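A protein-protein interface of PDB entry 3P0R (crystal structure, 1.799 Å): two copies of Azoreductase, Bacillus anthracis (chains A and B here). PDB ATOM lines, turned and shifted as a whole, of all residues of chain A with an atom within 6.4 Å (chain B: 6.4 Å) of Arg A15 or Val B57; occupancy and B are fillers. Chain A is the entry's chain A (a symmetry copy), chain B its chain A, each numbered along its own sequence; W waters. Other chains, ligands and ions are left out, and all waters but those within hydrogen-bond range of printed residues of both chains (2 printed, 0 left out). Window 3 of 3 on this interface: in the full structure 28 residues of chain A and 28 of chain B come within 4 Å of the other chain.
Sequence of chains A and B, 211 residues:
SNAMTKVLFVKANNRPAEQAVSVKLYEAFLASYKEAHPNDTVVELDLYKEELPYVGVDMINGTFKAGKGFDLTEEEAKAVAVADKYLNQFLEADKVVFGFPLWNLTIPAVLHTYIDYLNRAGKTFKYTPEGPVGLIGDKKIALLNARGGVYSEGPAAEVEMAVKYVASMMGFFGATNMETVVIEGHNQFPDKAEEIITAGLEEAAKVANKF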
ATOM      1  N   LYS A  11      12.969   2.476 -25.507  1.00  0.00           N
ATOM      2  CA  LYS A  11      11.896   2.885 -26.418  1.00  0.00           C
ATOM      3  C   LYS A  11      10.655   3.146 -25.616  1.00  0.00           C
ATOM      4  O   LYS A  11      10.255   2.325 -24.786  1.00  0.00           O
ATOM      5  CB  LYS A  11      11.596   1.772 -27.392  1.00  0.00           C
ATOM      6  CG  LYS A  11      10.616   2.133 -28.505  1.00  0.00           C
ATOM      7  CD  LYS A  11      10.237   0.939 -29.354  1.00  0.00           C
ATOM      8  CE  LYS A  11       9.311   1.326 -30.473  1.00  0.00           C
ATOM      9  NZ  LYS A  11       8.698   0.125 -31.144  1.00  0.00           N
ATOM     10  N   ASN A  13       7.260   4.257 -26.829  1.00  0.00           N
ATOM     11  CA  ASN A  13       6.110   4.492 -27.694  1.00  0.00           C
ATOM     12  C   ASN A  13       5.768   3.197 -28.420  1.00  0.00           C
ATOM     13  O   ASN A  13       6.570   2.725 -29.241  1.00  0.00           O
ATOM     14  CB  ASN A  13       6.420   5.579 -28.730  1.00  0.00           C
ATOM     15  CG  ASN A  13       5.165   6.108 -29.448  1.00  0.00           C
ATOM     16  OD1 ASN A  13       4.120   5.478 -29.445  1.00  0.00           O
ATOM     17  ND2 ASN A  13       5.280   7.307 -30.044  1.00  0.00           N
ATOM     18  N   ASN A  14       4.594   2.637 -28.130  1.00  0.00           N
ATOM     19  CA  ASN A  14       4.162   1.398 -28.709  1.00  0.00           C
ATOM     20  C   ASN A  14       3.194   1.586 -29.855  1.00  0.00           C
ATOM     21  O   ASN A  14       2.557   0.583 -30.292  1.00  0.00           O
ATOM     22  CB  ASN A  14       3.640   0.411 -27.667  1.00  0.00           C
ATOM     23  CG  ASN A  14       2.442   0.918 -26.888  1.00  0.00           C
ATOM     24  OD1 ASN A  14       2.059   2.056 -27.006  1.00  0.00           O
ATOM     25  ND2 ASN A  14       1.826   0.030 -26.118  1.00  0.00           N
ATOM     26  N   ARG A  15       3.085   2.830 -30.325  1.00  0.00           N
ATOM     27  CA  ARG A  15       2.319   3.096 -31.529  1.00  0.00           C
ATOM     28  C   ARG A  15       3.084   2.608 -32.733  1.00  0.00           C
ATOM     29  O   ARG A  15       4.322   2.551 -32.742  1.00  0.00           O
ATOM     30  CB  ARG A  15       1.954   4.574 -31.685  1.00  0.00           C
ATOM     31  CG  ARG A  15       1.096   5.130 -30.575  1.00  0.00           C
ATOM     32  CD  ARG A  15       0.802   6.617 -30.767  1.00  0.00           C
ATOM     33  NE  ARG A  15      -0.270   6.751 -31.762  1.00  0.00           N
ATOM     34  CZ  ARG A  15      -0.303   7.568 -32.808  1.00  0.00           C
ATOM     35  NH1 ARG A  15       0.676   8.431 -33.080  1.00  0.00           N
ATOM     36  NH2 ARG A  15      -1.376   7.524 -33.593  1.00  0.00           N
ATOM     37  N   PRO A  16       2.357   2.326 -33.808  1.00  0.00           N
ATOM     38  CA  PRO A  16       3.103   1.851 -34.973  1.00  0.00           C
ATOM     39  C   PRO A  16       3.931   2.960 -35.667  1.00  0.00           C
ATOM     40  O   PRO A  16       3.486   4.141 -35.726  1.00  0.00           O
ATOM     41  CB  PRO A  16       2.011   1.336 -35.890  1.00  0.00           C
ATOM     42  CG  PRO A  16       0.740   1.910 -35.418  1.00  0.00           C
ATOM     43  CD  PRO A  16       0.936   2.555 -34.081  1.00  0.00           C
ATOM     44  N   ALA A  17       5.090   2.586 -36.226  1.00  0.00           N
ATOM     45  CA  ALA A  17       5.955   3.520 -36.941  1.00  0.00           C
ATOM     46  C   ALA A  17       5.249   4.283 -38.020  1.00  0.00           C
ATOM     47  O   ALA A  17       5.637   5.410 -38.351  1.00  0.00           O
ATOM     48  CB  ALA A  17       7.127   2.786 -37.602  1.00  0.00           C
ATOM     49  N   GLU A  18       4.267   3.632 -38.622  1.00  0.00           N
ATOM     50  CA  GLU A  18       3.529   4.208 -39.739  1.00  0.00           C
ATOM     51  C   GLU A  18       2.799   5.478 -39.301  1.00  0.00           C
ATOM     52  O   GLU A  18       2.601   6.426 -40.109  1.00  0.00           O
ATOM     53  CB  GLU A  18       2.546   3.163 -40.278  1.00  0.00           C
ATOM     54  CG  GLU A  18       1.456   3.704 -41.162  1.00  0.00           C
ATOM     55  CD  GLU A  18       0.842   2.661 -42.038  1.00  0.00           C
ATOM     56  OE1 GLU A  18       0.572   1.532 -41.538  1.00  0.00           O
ATOM     57  OE2 GLU A  18       0.639   2.975 -43.234  1.00  0.00           O
ATOM     58  N   GLN A  19       2.378   5.482 -38.044  1.00  0.00           N
ATOM     59  CA  GLN A  19       1.676   6.612 -37.470  1.00  0.00           C
ATOM     60  C   GLN A  19       2.464   7.485 -36.508  1.00  0.00           C
ATOM     61  O   GLN A  19       1.988   8.582 -36.180  1.00  0.00           O
ATOM     62  CB  GLN A  19       0.460   6.133 -36.695  1.00  0.00           C
ATOM     63  CG  GLN A  19      -0.648   5.511 -37.500  1.00  0.00           C
ATOM     64  CD  GLN A  19      -1.810   5.194 -36.575  1.00  0.00           C
ATOM     65  OE1 GLN A  19      -1.651   4.421 -35.621  1.00  0.00           O
ATOM     66  NE2 GLN A  19      -2.950   5.811 -36.815  1.00  0.00           N
ATOM     67  N   ALA A  20       3.596   7.013 -35.995  1.00  0.00           N
ATOM     68  CA  ALA A  20       4.358   7.748 -34.994  1.00  0.00           C
ATOM     69  C   ALA A  20       5.730   8.121 -35.519  1.00  0.00           C
ATOM     70  O   ALA A  20       6.599   7.242 -35.626  1.00  0.00           O
ATOM     71  CB  ALA A  20       4.504   6.903 -33.730  1.00  0.00           C
ATOM     72  N   VAL A  21       5.940   9.410 -35.808  1.00  0.00           N
ATOM     73  CA  VAL A  21       7.240   9.853 -36.291  1.00  0.00           C
ATOM     74  C   VAL A  21       8.330   9.548 -35.245  1.00  0.00           C
ATOM     75  O   VAL A  21       9.479   9.250 -35.599  1.00  0.00           O
ATOM     76  CB  VAL A  21       7.189  11.358 -36.674  1.00  0.00           C
ATOM     77  CG1 VAL A  21       8.559  11.911 -36.960  1.00  0.00           C
ATOM     78  CG2 VAL A  21       6.294  11.511 -37.918  1.00  0.00           C
ATOM     79  N   VAL A  23       8.610   6.948 -33.405  1.00  0.00           N
ATOM     80  CA  VAL A  23       9.000   5.558 -33.626  1.00  0.00           C
ATOM     81  C   VAL A  23       9.816   5.409 -34.897  1.00  0.00           C
ATOM     82  O   VAL A  23      10.830   4.696 -34.931  1.00  0.00           O
ATOM     83  CB  VAL A  23       7.794   4.627 -33.627  1.00  0.00           C
ATOM     84  CG1 VAL A  23       8.210   3.206 -33.971  1.00  0.00           C
ATOM     85  CG2 VAL A  23       7.073   4.641 -32.229  1.00  0.00           C
ATOM     86  N   TYR A  48       6.983  -0.364 -22.859  1.00  0.00           N
ATOM     87  CA  TYR A  48       5.593  -0.859 -22.901  1.00  0.00           C
ATOM     88  C   TYR A  48       5.466  -2.361 -22.769  1.00  0.00           C
ATOM     89  O   TYR A  48       4.357  -2.863 -22.662  1.00  0.00           O
ATOM     90  CB  TYR A  48       4.854  -0.351 -24.148  1.00  0.00           C
ATOM     91  CG  TYR A  48       4.437   1.063 -23.988  1.00  0.00           C
ATOM     92  CD1 TYR A  48       3.295   1.389 -23.266  1.00  0.00           C
ATOM     93  CD2 TYR A  48       5.175   2.109 -24.561  1.00  0.00           C
ATOM     94  CE1 TYR A  48       2.911   2.723 -23.085  1.00  0.00           C
ATOM     95  CE2 TYR A  48       4.826   3.435 -24.364  1.00  0.00           C
ATOM     96  CZ  TYR A  48       3.673   3.741 -23.634  1.00  0.00           C
ATOM     97  OH  TYR A  48       3.290   5.042 -23.453  1.00  0.00           O
ATOM     98  N   TRP A 103       4.099  14.044 -25.585  1.00  0.00           N
ATOM     99  CA  TRP A 103       2.664  13.901 -25.395  1.00  0.00           C
ATOM    100  C   TRP A 103       2.264  14.722 -24.187  1.00  0.00           C
ATOM    101  O   TRP A 103       2.846  14.568 -23.115  1.00  0.00           O
ATOM    102  CB  TRP A 103       2.294  12.426 -25.110  1.00  0.00           C
ATOM    103  CG  TRP A 103       2.507  11.416 -26.213  1.00  0.00           C
ATOM    104  CD1 TRP A 103       2.629  11.641 -27.554  1.00  0.00           C
ATOM    105  CD2 TRP A 103       2.457   9.994 -26.058  1.00  0.00           C
ATOM    106  NE1 TRP A 103       2.708  10.450 -28.221  1.00  0.00           N
ATOM    107  CE2 TRP A 103       2.637   9.426 -27.326  1.00  0.00           C
ATOM    108  CE3 TRP A 103       2.342   9.156 -24.962  1.00  0.00           C
ATOM    109  CZ2 TRP A 103       2.689   8.028 -27.528  1.00  0.00           C
ATOM    110  CZ3 TRP A 103       2.367   7.764 -25.174  1.00  0.00           C
ATOM    111  CH2 TRP A 103       2.537   7.234 -26.448  1.00  0.00           C
ATOM    112  N   VAL B  55      -0.825   5.188 -20.261  1.00  0.00           N
ATOM    113  CA  VAL B  55      -1.273   5.533 -21.604  1.00  0.00           C
ATOM    114  C   VAL B  55      -0.288   5.102 -22.686  1.00  0.00           C
ATOM    115  O   VAL B  55       0.891   5.541 -22.727  1.00  0.00           O
ATOM    116  CB  VAL B  55      -1.570   7.042 -21.712  1.00  0.00           C
ATOM    117  CG1 VAL B  55      -1.971   7.421 -23.127  1.00  0.00           C
ATOM    118  CG2 VAL B  55      -2.744   7.402 -20.767  1.00  0.00           C
ATOM    119  N   GLY B  56      -0.806   4.258 -23.560  1.00  0.00           N
ATOM    120  CA  GLY B  56      -0.085   3.794 -24.723  1.00  0.00           C
ATOM    121  C   GLY B  56      -1.076   3.633 -25.867  1.00  0.00           C
ATOM    122  O   GLY B  56      -2.185   4.172 -25.812  1.00  0.00           O
ATOM    123  N   VAL B  57      -0.691   2.832 -26.859  1.00  0.00           N
ATOM    124  CA  VAL B  57      -1.448   2.733 -28.104  1.00  0.00           C
ATOM    125  C   VAL B  57      -2.903   2.283 -27.849  1.00  0.00           C
ATOM    126  O   VAL B  57      -3.814   2.755 -28.524  1.00  0.00           O
ATOM    127  CB  VAL B  57      -0.719   1.809 -29.096  1.00  0.00           C
ATOM    128  CG1 VAL B  57      -0.701   0.371 -28.599  1.00  0.00           C
ATOM    129  CG2 VAL B  57      -1.266   1.915 -30.499  1.00  0.00           C
ATOM    130  N   ASP B  58      -3.136   1.379 -26.898  1.00  0.00           N
ATOM    131  CA  ASP B  58      -4.510   0.882 -26.693  1.00  0.00           C
ATOM    132  C   ASP B  58      -5.424   2.033 -26.218  1.00  0.00           C
ATOM    133  O   ASP B  58      -6.555   2.177 -26.673  1.00  0.00           O
ATOM    134  CB  ASP B  58      -4.573  -0.337 -25.746  1.00  0.00           C
ATOM    135  CG  ASP B  58      -4.022  -1.607 -26.377  1.00  0.00           C
ATOM    136  OD1 ASP B  58      -4.000  -1.687 -27.597  1.00  0.00           O
ATOM    137  OD2 ASP B  58      -3.562  -2.508 -25.637  1.00  0.00           O
ATOM    138  N   MET B  59      -4.895   2.857 -25.319  1.00  0.00           N
ATOM    139  CA  MET B  59      -5.641   3.985 -24.777  1.00  0.00           C
ATOM    140  C   MET B  59      -5.769   5.134 -25.774  1.00  0.00           C
ATOM    141  O   MET B  59      -6.699   5.936 -25.684  1.00  0.00           O
ATOM    142  CB  MET B  59      -4.990   4.483 -23.485  1.00  0.00           C
ATOM    143  CG  MET B  59      -5.457   5.862 -23.046  1.00  0.00           C
ATOM    144  SD  MET B  59      -7.028   5.792 -21.892  1.00  0.00           S
ATOM    145  CE  MET B  59      -6.137   5.466 -20.189  1.00  0.00           C
ATOM    146  N   ILE B  60      -4.839   5.220 -26.721  1.00  0.00           N
ATOM    147  CA  ILE B  60      -4.862   6.295 -27.681  1.00  0.00           C
ATOM    148  C   ILE B  60      -5.812   5.924 -28.815  1.00  0.00           C
ATOM    149  O   ILE B  60      -6.681   6.716 -29.164  1.00  0.00           O
ATOM    150  CB  ILE B  60      -3.448   6.611 -28.178  1.00  0.00           C
ATOM    151  CG1 ILE B  60      -2.658   7.295 -27.017  1.00  0.00           C
ATOM    152  CG2 ILE B  60      -3.523   7.515 -29.407  1.00  0.00           C
ATOM    153  CD1 ILE B  60      -1.082   7.351 -27.228  1.00  0.00           C
ATOM    154  N   ASN B  61      -5.626   4.735 -29.399  1.00  0.00           N
ATOM    155  CA  ASN B  61      -6.543   4.197 -30.409  1.00  0.00           C
ATOM    156  C   ASN B  61      -7.946   4.040 -29.867  1.00  0.00           C
ATOM    157  O   ASN B  61      -8.926   4.362 -30.549  1.00  0.00           O
ATOM    158  CB  ASN B  61      -6.047   2.841 -30.914  1.00  0.00           C
ATOM    159  CG  ASN B  61      -4.845   2.982 -31.793  1.00  0.00           C
ATOM    160  OD1 ASN B  61      -4.480   4.100 -32.131  1.00  0.00           O
ATOM    161  ND2 ASN B  61      -4.215   1.877 -32.168  1.00  0.00           N
ATOM    162  N   GLY B  62      -8.008   3.522 -28.646  1.00  0.00           N
ATOM    163  CA  GLY B  62      -9.259   3.248 -27.953  1.00  0.00           C
ATOM    164  C   GLY B  62     -10.120   4.494 -27.841  1.00  0.00           C
ATOM    165  O   GLY B  62     -11.321   4.468 -28.239  1.00  0.00           O
ATOM    166  N   GLU B  76      -8.581  -2.160 -25.628  1.00  0.00           N
ATOM    167  CA  GLU B  76      -8.880  -0.770 -25.969  1.00  0.00           C
ATOM    168  C   GLU B  76     -10.060  -0.290 -25.126  1.00  0.00           C
ATOM    169  O   GLU B  76      -9.997   0.773 -24.538  1.00  0.00           O
ATOM    170  CB  GLU B  76      -9.176  -0.626 -27.462  1.00  0.00           C
ATOM    171  CG  GLU B  76      -7.894  -0.615 -28.365  1.00  0.00           C
ATOM    172  CD  GLU B  76      -8.199  -0.723 -29.858  1.00  0.00           C
ATOM    173  OE1 GLU B  76      -9.371  -0.964 -30.215  1.00  0.00           O
ATOM    174  OE2 GLU B  76      -7.257  -0.576 -30.679  1.00  0.00           O
HETATM  175  O   HOH W   1       2.933   6.257 -20.391  1.00  0.00           O
HETATM  176  O   HOH W   2      -2.243   4.867 -32.555  1.00  0.00           O
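O of Val B55 is in hydrogen-bond range of OH of Tyr A48, 2.6 Å away. N of Val B57 is in hydrogen-bond range of OD1 of Asn A14 (2.9 Å).
The side-chain amide oxygen (OD1) of Asn A13 sits at hydrogen-bond distance from the backbone NH (N) of Arg A15 (3.0 Å). NH1 of Arg A15 sits at hydrogen-bond distance from O of Gln A19 (3.4 Å).
Asn A14 touches Gly B56. Arg A15 touches Val B57 (CA to CG2, 3.9 Å). Gly B56 touches Tyr A48. Trp A103 touches Val B55 (CZ3 to O, 3.6 Å). Ile B60 touches Trp A103 (CD1 to CH2, 3.7 Å).
Of the printed residues of chain B, Arg A15 touches Val B57 (3.9 Å). Of chain A, only Asn A14 (2.9 Å) and Arg A15 (3.9 Å) come within 4 Å of Val B57. Of the printed residues of chain A, Val B55 touches Tyr A48 (2.6 Å) and Trp A103 (3.6 Å). Printed residues of chain A within 4 Å of Ile B60: Trp A103. Printed residues of chain B within 4 Å of Asn A14: Gly B56 and Val B57. Of the printed residues of chain A, Gly B56 touches Asn A14 (3.6 Å) and Tyr A48 (3.6 Å). Asn A13 touches none of the printed residues of chain B. The nearest residue of chain B that does not touch Arg A15 is Ile B60 (4.1 Å). The nearest residue of chain A that does not touch Val B57 is Pro A16 (4.3 Å).
Of the 13 printed residues of chain A, 4 touch a printed residue of chain B. Hydrophobic or aromatic side chains of chain A within 4 Å of the printed part of chain B: Tyr A48 and Trp A103. Along chain A the printed residues that touch a printed residue of chain B span positions 14 to 103. Among the printed residues, 7 pairs touch across the chains.
No position is printed for both chains. Of the 7 pairs that touch across the chains among the printed residues, none has its exchanged pair printed and touching as well.
Water W2 lies within hydrogen-bond range of the side-chain amide oxygen of Asn B61 (2.4 Å), the guanidinium group of Arg A15 (2.8 Å) and the side-chain amide oxygen of Gln A19 (3.2 Å). Water W1 lies within hydrogen-bond range of O of Val B55 (3.2 Å) and OH of Tyr A48 (3.3 Å).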
